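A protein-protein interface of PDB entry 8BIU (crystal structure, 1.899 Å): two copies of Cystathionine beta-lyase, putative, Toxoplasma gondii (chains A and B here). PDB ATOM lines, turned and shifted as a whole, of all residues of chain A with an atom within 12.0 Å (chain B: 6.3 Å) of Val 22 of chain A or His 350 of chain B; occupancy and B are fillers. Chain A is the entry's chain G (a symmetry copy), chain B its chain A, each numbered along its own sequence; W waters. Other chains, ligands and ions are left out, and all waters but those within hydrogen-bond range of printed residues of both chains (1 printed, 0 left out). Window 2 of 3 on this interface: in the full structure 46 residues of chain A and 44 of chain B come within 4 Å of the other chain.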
ATOM      1  N   VAL A  22      33.913  -8.574 -18.692  1.00  0.00           N
ATOM      2  CA  VAL A  22      32.499  -8.897 -18.541  1.00  0.00           C
ATOM      3  C   VAL A  22      31.643  -7.868 -19.290  1.00  0.00           C
ATOM      4  O   VAL A  22      31.708  -6.671 -19.008  1.00  0.00           O
ATOM      5  CB  VAL A  22      32.115  -8.981 -17.047  1.00  0.00           C
ATOM      6  CG1 VAL A  22      30.685  -9.482 -16.877  1.00  0.00           C
ATOM      7  CG2 VAL A  22      33.088  -9.890 -16.315  1.00  0.00           C
ATOM      8  N   LYS A  23      30.862  -8.351 -20.257  1.00  0.00           N
ATOM      9  CA  LYS A  23      30.027  -7.518 -21.110  1.00  0.00           C
ATOM     10  C   LYS A  23      28.566  -7.590 -20.676  1.00  0.00           C
ATOM     11  O   LYS A  23      28.195  -8.320 -19.751  1.00  0.00           O
ATOM     12  CB  LYS A  23      30.166  -7.943 -22.575  1.00  0.00           C
ATOM     13  N   ALA A  24      27.730  -6.811 -21.366  1.00  0.00           N
ATOM     14  CA  ALA A  24      26.298  -6.833 -21.111  1.00  0.00           C
ATOM     15  C   ALA A  24      25.764  -8.255 -21.216  1.00  0.00           C
ATOM     16  O   ALA A  24      26.156  -9.017 -22.103  1.00  0.00           O
ATOM     17  CB  ALA A  24      25.576  -5.914 -22.098  1.00  0.00           C
ATOM     18  N   GLY A  25      24.880  -8.617 -20.289  1.00  0.00           N
ATOM     19  CA  GLY A  25      24.242  -9.914 -20.291  1.00  0.00           C
ATOM     20  C   GLY A  25      24.905 -10.964 -19.425  1.00  0.00           C
ATOM     21  O   GLY A  25      24.365 -12.072 -19.308  1.00  0.00           O
ATOM     22  N   ASP A  26      26.049 -10.664 -18.827  1.00  0.00           N
ATOM     23  CA  ASP A  26      26.764 -11.606 -17.982  1.00  0.00           C
ATOM     24  C   ASP A  26      26.653 -11.174 -16.524  1.00  0.00           C
ATOM     25  O   ASP A  26      26.644  -9.979 -16.228  1.00  0.00           O
ATOM     26  CB  ASP A  26      28.249 -11.684 -18.378  1.00  0.00           C
ATOM     27  CG  ASP A  26      28.469 -12.138 -19.822  1.00  0.00           C
ATOM     28  OD1 ASP A  26      29.563 -11.853 -20.371  1.00  0.00           O
ATOM     29  OD2 ASP A  26      27.576 -12.798 -20.402  1.00  0.00           O
ATOM     30  N   TRP A  27      26.569 -12.148 -15.616  1.00  0.00           N
ATOM     31  CA  TRP A  27      26.802 -11.867 -14.205  1.00  0.00           C
ATOM     32  C   TRP A  27      28.301 -11.724 -13.959  1.00  0.00           C
ATOM     33  O   TRP A  27      29.118 -12.417 -14.569  1.00  0.00           O
ATOM     34  CB  TRP A  27      26.256 -12.982 -13.306  1.00  0.00           C
ATOM     35  CG  TRP A  27      24.780 -13.269 -13.431  1.00  0.00           C
ATOM     36  CD1 TRP A  27      24.200 -14.199 -14.239  1.00  0.00           C
ATOM     37  CD2 TRP A  27      23.710 -12.645 -12.707  1.00  0.00           C
ATOM     38  NE1 TRP A  27      22.839 -14.182 -14.081  1.00  0.00           N
ATOM     39  CE2 TRP A  27      22.511 -13.238 -13.145  1.00  0.00           C
ATOM     40  CE3 TRP A  27      23.648 -11.638 -11.741  1.00  0.00           C
ATOM     41  CZ2 TRP A  27      21.260 -12.855 -12.648  1.00  0.00           C
ATOM     42  CZ3 TRP A  27      22.404 -11.264 -11.246  1.00  0.00           C
ATOM     43  CH2 TRP A  27      21.230 -11.867 -11.703  1.00  0.00           C
ATOM     44  N   LEU A  28      28.667 -10.828 -13.050  1.00  0.00           N
ATOM     45  CA  LEU A  28      30.079 -10.686 -12.723  1.00  0.00           C
ATOM     46  C   LEU A  28      30.610 -11.993 -12.141  1.00  0.00           C
ATOM     47  O   LEU A  28      30.044 -12.509 -11.165  1.00  0.00           O
ATOM     48  CB  LEU A  28      30.317  -9.548 -11.736  1.00  0.00           C
ATOM     49  CG  LEU A  28      29.883  -8.158 -12.187  1.00  0.00           C
ATOM     50  CD1 LEU A  28      29.771  -7.216 -10.991  1.00  0.00           C
ATOM     51  CD2 LEU A  28      30.840  -7.623 -13.229  1.00  0.00           C
ATOM     52  N   PRO A  29      31.683 -12.552 -12.693  1.00  0.00           N
ATOM     53  CA  PRO A  29      32.240 -13.781 -12.120  1.00  0.00           C
ATOM     54  C   PRO A  29      32.634 -13.563 -10.670  1.00  0.00           C
ATOM     55  O   PRO A  29      33.187 -12.525 -10.313  1.00  0.00           O
ATOM     56  CB  PRO A  29      33.458 -14.073 -13.007  1.00  0.00           C
ATOM     57  CG  PRO A  29      33.283 -13.210 -14.227  1.00  0.00           C
ATOM     58  CD  PRO A  29      32.532 -12.009 -13.764  1.00  0.00           C
ATOM     59  N   GLY A  30      32.330 -14.551  -9.830  1.00  0.00           N
ATOM     60  CA  GLY A  30      32.706 -14.516  -8.434  1.00  0.00           C
ATOM     61  C   GLY A  30      31.736 -13.798  -7.523  1.00  0.00           C
ATOM     62  O   GLY A  30      31.926 -13.820  -6.304  1.00  0.00           O
ATOM     63  N   PHE A  31      30.710 -13.164  -8.066  1.00  0.00           N
ATOM     64  CA  PHE A  31      29.729 -12.486  -7.241  1.00  0.00           C
ATOM     65  C   PHE A  31      28.446 -13.290  -7.152  1.00  0.00           C
ATOM     66  O   PHE A  31      28.044 -13.965  -8.098  1.00  0.00           O
ATOM     67  CB  PHE A  31      29.421 -11.095  -7.782  1.00  0.00           C
ATOM     68  CG  PHE A  31      30.559 -10.150  -7.664  1.00  0.00           C
ATOM     69  CD1 PHE A  31      30.601  -9.243  -6.629  1.00  0.00           C
ATOM     70  CD2 PHE A  31      31.581 -10.163  -8.578  1.00  0.00           C
ATOM     71  CE1 PHE A  31      31.652  -8.367  -6.509  1.00  0.00           C
ATOM     72  CE2 PHE A  31      32.629  -9.280  -8.466  1.00  0.00           C
ATOM     73  CZ  PHE A  31      32.666  -8.385  -7.429  1.00  0.00           C
ATOM     74  N   THR A  32      27.803 -13.189  -5.995  1.00  0.00           N
ATOM     75  CA  THR A  32      26.545 -13.850  -5.710  1.00  0.00           C
ATOM     76  C   THR A  32      25.443 -12.805  -5.634  1.00  0.00           C
ATOM     77  O   THR A  32      25.559 -11.859  -4.837  1.00  0.00           O
ATOM     78  CB  THR A  32      26.650 -14.620  -4.397  1.00  0.00           C
ATOM     79  OG1 THR A  32      27.670 -15.620  -4.528  1.00  0.00           O
ATOM     80  CG2 THR A  32      25.336 -15.288  -4.059  1.00  0.00           C
ATOM     81  N   ILE B 345      28.782   4.328 -24.832  1.00  0.00           N
ATOM     82  CA  ILE B 345      28.680   3.033 -25.494  1.00  0.00           C
ATOM     83  C   ILE B 345      29.508   1.983 -24.774  1.00  0.00           C
ATOM     84  O   ILE B 345      29.065   0.845 -24.608  1.00  0.00           O
ATOM     85  CB  ILE B 345      29.094   3.161 -26.967  1.00  0.00           C
ATOM     86  CG1 ILE B 345      28.101   4.053 -27.714  1.00  0.00           C
ATOM     87  CG2 ILE B 345      29.200   1.789 -27.601  1.00  0.00           C
ATOM     88  CD1 ILE B 345      26.679   3.859 -27.262  1.00  0.00           C
ATOM     89  N   ARG B 346      30.727   2.326 -24.357  1.00  0.00           N
ATOM     90  CA  ARG B 346      31.500   1.390 -23.539  1.00  0.00           C
ATOM     91  C   ARG B 346      30.737   1.026 -22.271  1.00  0.00           C
ATOM     92  O   ARG B 346      30.669  -0.149 -21.878  1.00  0.00           O
ATOM     93  CB  ARG B 346      32.864   1.991 -23.192  1.00  0.00           C
ATOM     94  CG  ARG B 346      33.884   1.904 -24.315  1.00  0.00           C
ATOM     95  CD  ARG B 346      35.323   2.052 -23.817  1.00  0.00           C
ATOM     96  NE  ARG B 346      35.524   3.293 -23.072  1.00  0.00           N
ATOM     97  CZ  ARG B 346      35.521   4.507 -23.616  1.00  0.00           C
ATOM     98  NH1 ARG B 346      35.326   4.655 -24.920  1.00  0.00           N
ATOM     99  NH2 ARG B 346      35.710   5.580 -22.855  1.00  0.00           N
ATOM    100  N   MET B 347      30.144   2.029 -21.624  1.00  0.00           N
ATOM    101  CA  MET B 347      29.384   1.797 -20.404  1.00  0.00           C
ATOM    102  C   MET B 347      28.221   0.846 -20.657  1.00  0.00           C
ATOM    103  O   MET B 347      28.072  -0.170 -19.971  1.00  0.00           O
ATOM    104  CB  MET B 347      28.899   3.139 -19.862  1.00  0.00           C
ATOM    105  CG  MET B 347      28.615   3.174 -18.370  1.00  0.00           C
ATOM    106  SD  MET B 347      26.847   3.083 -18.123  1.00  0.00           S
ATOM    107  CE  MET B 347      26.410   4.781 -18.420  1.00  0.00           C
ATOM    108  N   MET B 348      27.388   1.158 -21.649  1.00  0.00           N
ATOM    109  CA  MET B 348      26.286   0.274 -22.010  1.00  0.00           C
ATOM    110  C   MET B 348      26.776  -1.137 -22.302  1.00  0.00           C
ATOM    111  O   MET B 348      26.228  -2.115 -21.781  1.00  0.00           O
ATOM    112  CB  MET B 348      25.531   0.840 -23.213  1.00  0.00           C
ATOM    113  CG  MET B 348      24.711   2.056 -22.877  1.00  0.00           C
ATOM    114  SD  MET B 348      23.275   1.581 -21.911  1.00  0.00           S
ATOM    115  CE  MET B 348      23.979   1.668 -20.262  1.00  0.00           C
ATOM    116  N   ASN B 349      27.805  -1.267 -23.142  1.00  0.00           N
ATOM    117  CA  ASN B 349      28.310  -2.586 -23.483  1.00  0.00           C
ATOM    118  C   ASN B 349      28.904  -3.310 -22.288  1.00  0.00           C
ATOM    119  O   ASN B 349      29.177  -4.508 -22.392  1.00  0.00           O
ATOM    120  CB  ASN B 349      29.359  -2.487 -24.588  1.00  0.00           C
ATOM    121  CG  ASN B 349      28.761  -2.080 -25.915  1.00  0.00           C
ATOM    122  OD1 ASN B 349      27.540  -2.053 -26.076  1.00  0.00           O
ATOM    123  ND2 ASN B 349      29.615  -1.772 -26.881  1.00  0.00           N
ATOM    124  N   HIS B 350      29.119  -2.628 -21.166  1.00  0.00           N
ATOM    125  CA  HIS B 350      29.722  -3.282 -20.014  1.00  0.00           C
ATOM    126  C   HIS B 350      28.816  -3.348 -18.791  1.00  0.00           C
ATOM    127  O   HIS B 350      29.276  -3.787 -17.731  1.00  0.00           O
ATOM    128  CB  HIS B 350      31.046  -2.594 -19.656  1.00  0.00           C
ATOM    129  CG  HIS B 350      32.099  -2.753 -20.708  1.00  0.00           C
ATOM    130  ND1 HIS B 350      32.117  -2.004 -21.864  1.00  0.00           N
ATOM    131  CD2 HIS B 350      33.147  -3.607 -20.798  1.00  0.00           C
ATOM    132  CE1 HIS B 350      33.138  -2.377 -22.613  1.00  0.00           C
ATOM    133  NE2 HIS B 350      33.779  -3.349 -21.990  1.00  0.00           N
ATOM    134  N   VAL B 351      27.553  -2.947 -18.889  1.00  0.00           N
ATOM    135  CA  VAL B 351      26.674  -3.055 -17.723  1.00  0.00           C
ATOM    136  C   VAL B 351      26.271  -4.533 -17.553  1.00  0.00           C
ATOM    137  O   VAL B 351      25.779  -5.138 -18.507  1.00  0.00           O
ATOM    138  CB  VAL B 351      25.446  -2.162 -17.853  1.00  0.00           C
ATOM    139  CG1 VAL B 351      24.430  -2.727 -18.833  1.00  0.00           C
ATOM    140  CG2 VAL B 351      24.800  -1.947 -16.488  1.00  0.00           C
ATOM    141  N   PRO B 352      26.522  -5.116 -16.422  1.00  0.00           N
ATOM    142  CA  PRO B 352      26.290  -6.556 -16.294  1.00  0.00           C
ATOM    143  C   PRO B 352      24.892  -6.872 -15.796  1.00  0.00           C
ATOM    144  O   PRO B 352      24.115  -5.969 -15.467  1.00  0.00           O
ATOM    145  CB  PRO B 352      27.360  -6.967 -15.278  1.00  0.00           C
ATOM    146  CG  PRO B 352      27.434  -5.776 -14.360  1.00  0.00           C
ATOM    147  CD  PRO B 352      27.146  -4.552 -15.210  1.00  0.00           C
ATOM    148  N   GLY B 409      26.456  -3.020 -10.386  1.00  0.00           N
ATOM    149  CA  GLY B 409      26.548  -3.145 -11.830  1.00  0.00           C
ATOM    150  C   GLY B 409      26.760  -1.813 -12.523  1.00  0.00           C
ATOM    151  O   GLY B 409      27.569  -1.706 -13.449  1.00  0.00           O
ATOM    152  N   TYR B 412      30.457  -0.757 -11.819  1.00  0.00           N
ATOM    153  CA  TYR B 412      31.350  -1.493 -12.707  1.00  0.00           C
ATOM    154  C   TYR B 412      31.319  -0.905 -14.108  1.00  0.00           C
ATOM    155  O   TYR B 412      32.357  -0.519 -14.656  1.00  0.00           O
ATOM    156  CB  TYR B 412      30.949  -2.969 -12.746  1.00  0.00           C
ATOM    157  CG  TYR B 412      31.689  -3.780 -13.792  1.00  0.00           C
ATOM    158  CD1 TYR B 412      32.887  -4.412 -13.486  1.00  0.00           C
ATOM    159  CD2 TYR B 412      31.190  -3.912 -15.082  1.00  0.00           C
ATOM    160  CE1 TYR B 412      33.572  -5.150 -14.428  1.00  0.00           C
ATOM    161  CE2 TYR B 412      31.865  -4.646 -16.033  1.00  0.00           C
ATOM    162  CZ  TYR B 412      33.060  -5.264 -15.701  1.00  0.00           C
ATOM    163  OH  TYR B 412      33.745  -5.991 -16.641  1.00  0.00           O
ATOM    164  N   ALA B 413      30.129  -0.853 -14.713  1.00  0.00           N
ATOM    165  CA  ALA B 413      30.017  -0.327 -16.065  1.00  0.00           C
ATOM    166  C   ALA B 413      30.673   1.038 -16.177  1.00  0.00           C
ATOM    167  O   ALA B 413      31.339   1.324 -17.175  1.00  0.00           O
ATOM    168  CB  ALA B 413      28.550  -0.249 -16.477  1.00  0.00           C
ATOM    169  N   LYS B 416      34.247   1.080 -16.317  1.00  0.00           N
ATOM    170  CA  LYS B 416      34.615   0.618 -17.649  1.00  0.00           C
ATOM    171  C   LYS B 416      34.415   1.687 -18.717  1.00  0.00           C
ATOM    172  O   LYS B 416      35.070   1.641 -19.765  1.00  0.00           O
ATOM    173  CB  LYS B 416      33.797  -0.618 -18.006  1.00  0.00           C
ATOM    174  CG  LYS B 416      34.338  -1.890 -17.443  1.00  0.00           C
ATOM    175  CD  LYS B 416      35.675  -2.174 -18.062  1.00  0.00           C
ATOM    176  CE  LYS B 416      36.522  -3.014 -17.154  1.00  0.00           C
ATOM    177  NZ  LYS B 416      37.626  -3.664 -17.918  1.00  0.00           N
ATOM    178  N   ALA B 417      33.517   2.634 -18.486  1.00  0.00           N
ATOM    179  CA  ALA B 417      33.195   3.642 -19.486  1.00  0.00           C
ATOM    180  C   ALA B 417      34.442   4.378 -19.970  1.00  0.00           C
ATOM    181  O   ALA B 417      34.443   4.938 -21.067  1.00  0.00           O
ATOM    182  CB  ALA B 417      32.187   4.628 -18.930  1.00  0.00           C
ATOM    183  OXT ALA B 417      35.473   4.440 -19.292  1.00  0.00           O
HETATM  184  O   HOH W   1      23.224  -6.685 -18.927  1.00  0.00           O
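The side-chain hydroxyl (OH) of Tyr 412 of chain B is in hydrogen-bond range of the backbone carbonyl oxygen (O) of Val 22 of chain A, at 3.2 Å. The backbone NH (N) of Ala 24 of chain A is in hydrogen-bond range of the backbone carbonyl oxygen (O) of Asn 349 of chain B (2.9 Å).
His 350 of chain B touches Val 22 of chain A. Lys 23 of chain A touches Asn 349 of chain B (CA to O, 3.4 Å). Ala 24 of chain A touches Met 348 of chain B. Val 351 of chain B touches Ala 24 of chain A. Pro 352 of chain B touches Asp 26 of chain A. Tyr 412 of chain B touches Leu 28 of chain A.
No position is printed for both chains.
Of the printed residues of chain B, Val 22 of chain A touches His 350 (3.8 Å) and Tyr 412 (3.2 Å). Of chain A, only Val 22 comes within 4 Å of His 350 of chain B. Of the printed residues of chain A, Met 348 of chain B touches Ala 24 (3.9 Å). Of the printed residues of chain A, Asn 349 of chain B touches Lys 23 (3.4 Å) and Ala 24 (2.9 Å). Pro 352 of chain B touches just one residue of chain A: Asp 26. Gly 409 of chain B touches none of the printed residues of chain A. Of chain A, only Val 22 and Leu 28 come within 4 Å of Tyr 412 of chain B. No residue of chain A comes within 4 Å of Ala 417 of chain B. Of the printed residues of chain B, Ala 24 of chain A touches Met 348, Asn 349 and Val 351. Printed residues of chain B within 4 Å of Asp 26 of chain A: Pro 352. Printed residues of chain B within 4 Å of Leu 28 of chain A: Tyr 412 (3.8 Å). Trp 27 of chain A touches none of the printed residues of chain B. Met 347 of chain B touches none of the printed residues of chain A.
Of the 13 printed residues of chain B, 6 touch a printed residue of chain A. Printed residues of chain B that touch a printed residue of chain A: Met 348, Asn 349, His 350, Val 351, Pro 352 and Tyr 412. Hydrophobic or aromatic side chains of chain B that line the printed part of chain A: His 350, Pro 352 and Tyr 412. Among the printed residues, 8 pairs touch across the chains. Among the printed residues, no Asp or Glu carboxylate lies within 4 Å of a Lys or Arg side-chain nitrogen of the other chain.
Water W1 lies within hydrogen-bond range of the backbone NH of Gly 25 of chain A (2.9 Å) and the backbone carbonyl oxygen of Val 351 of chain B (3.0 Å).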
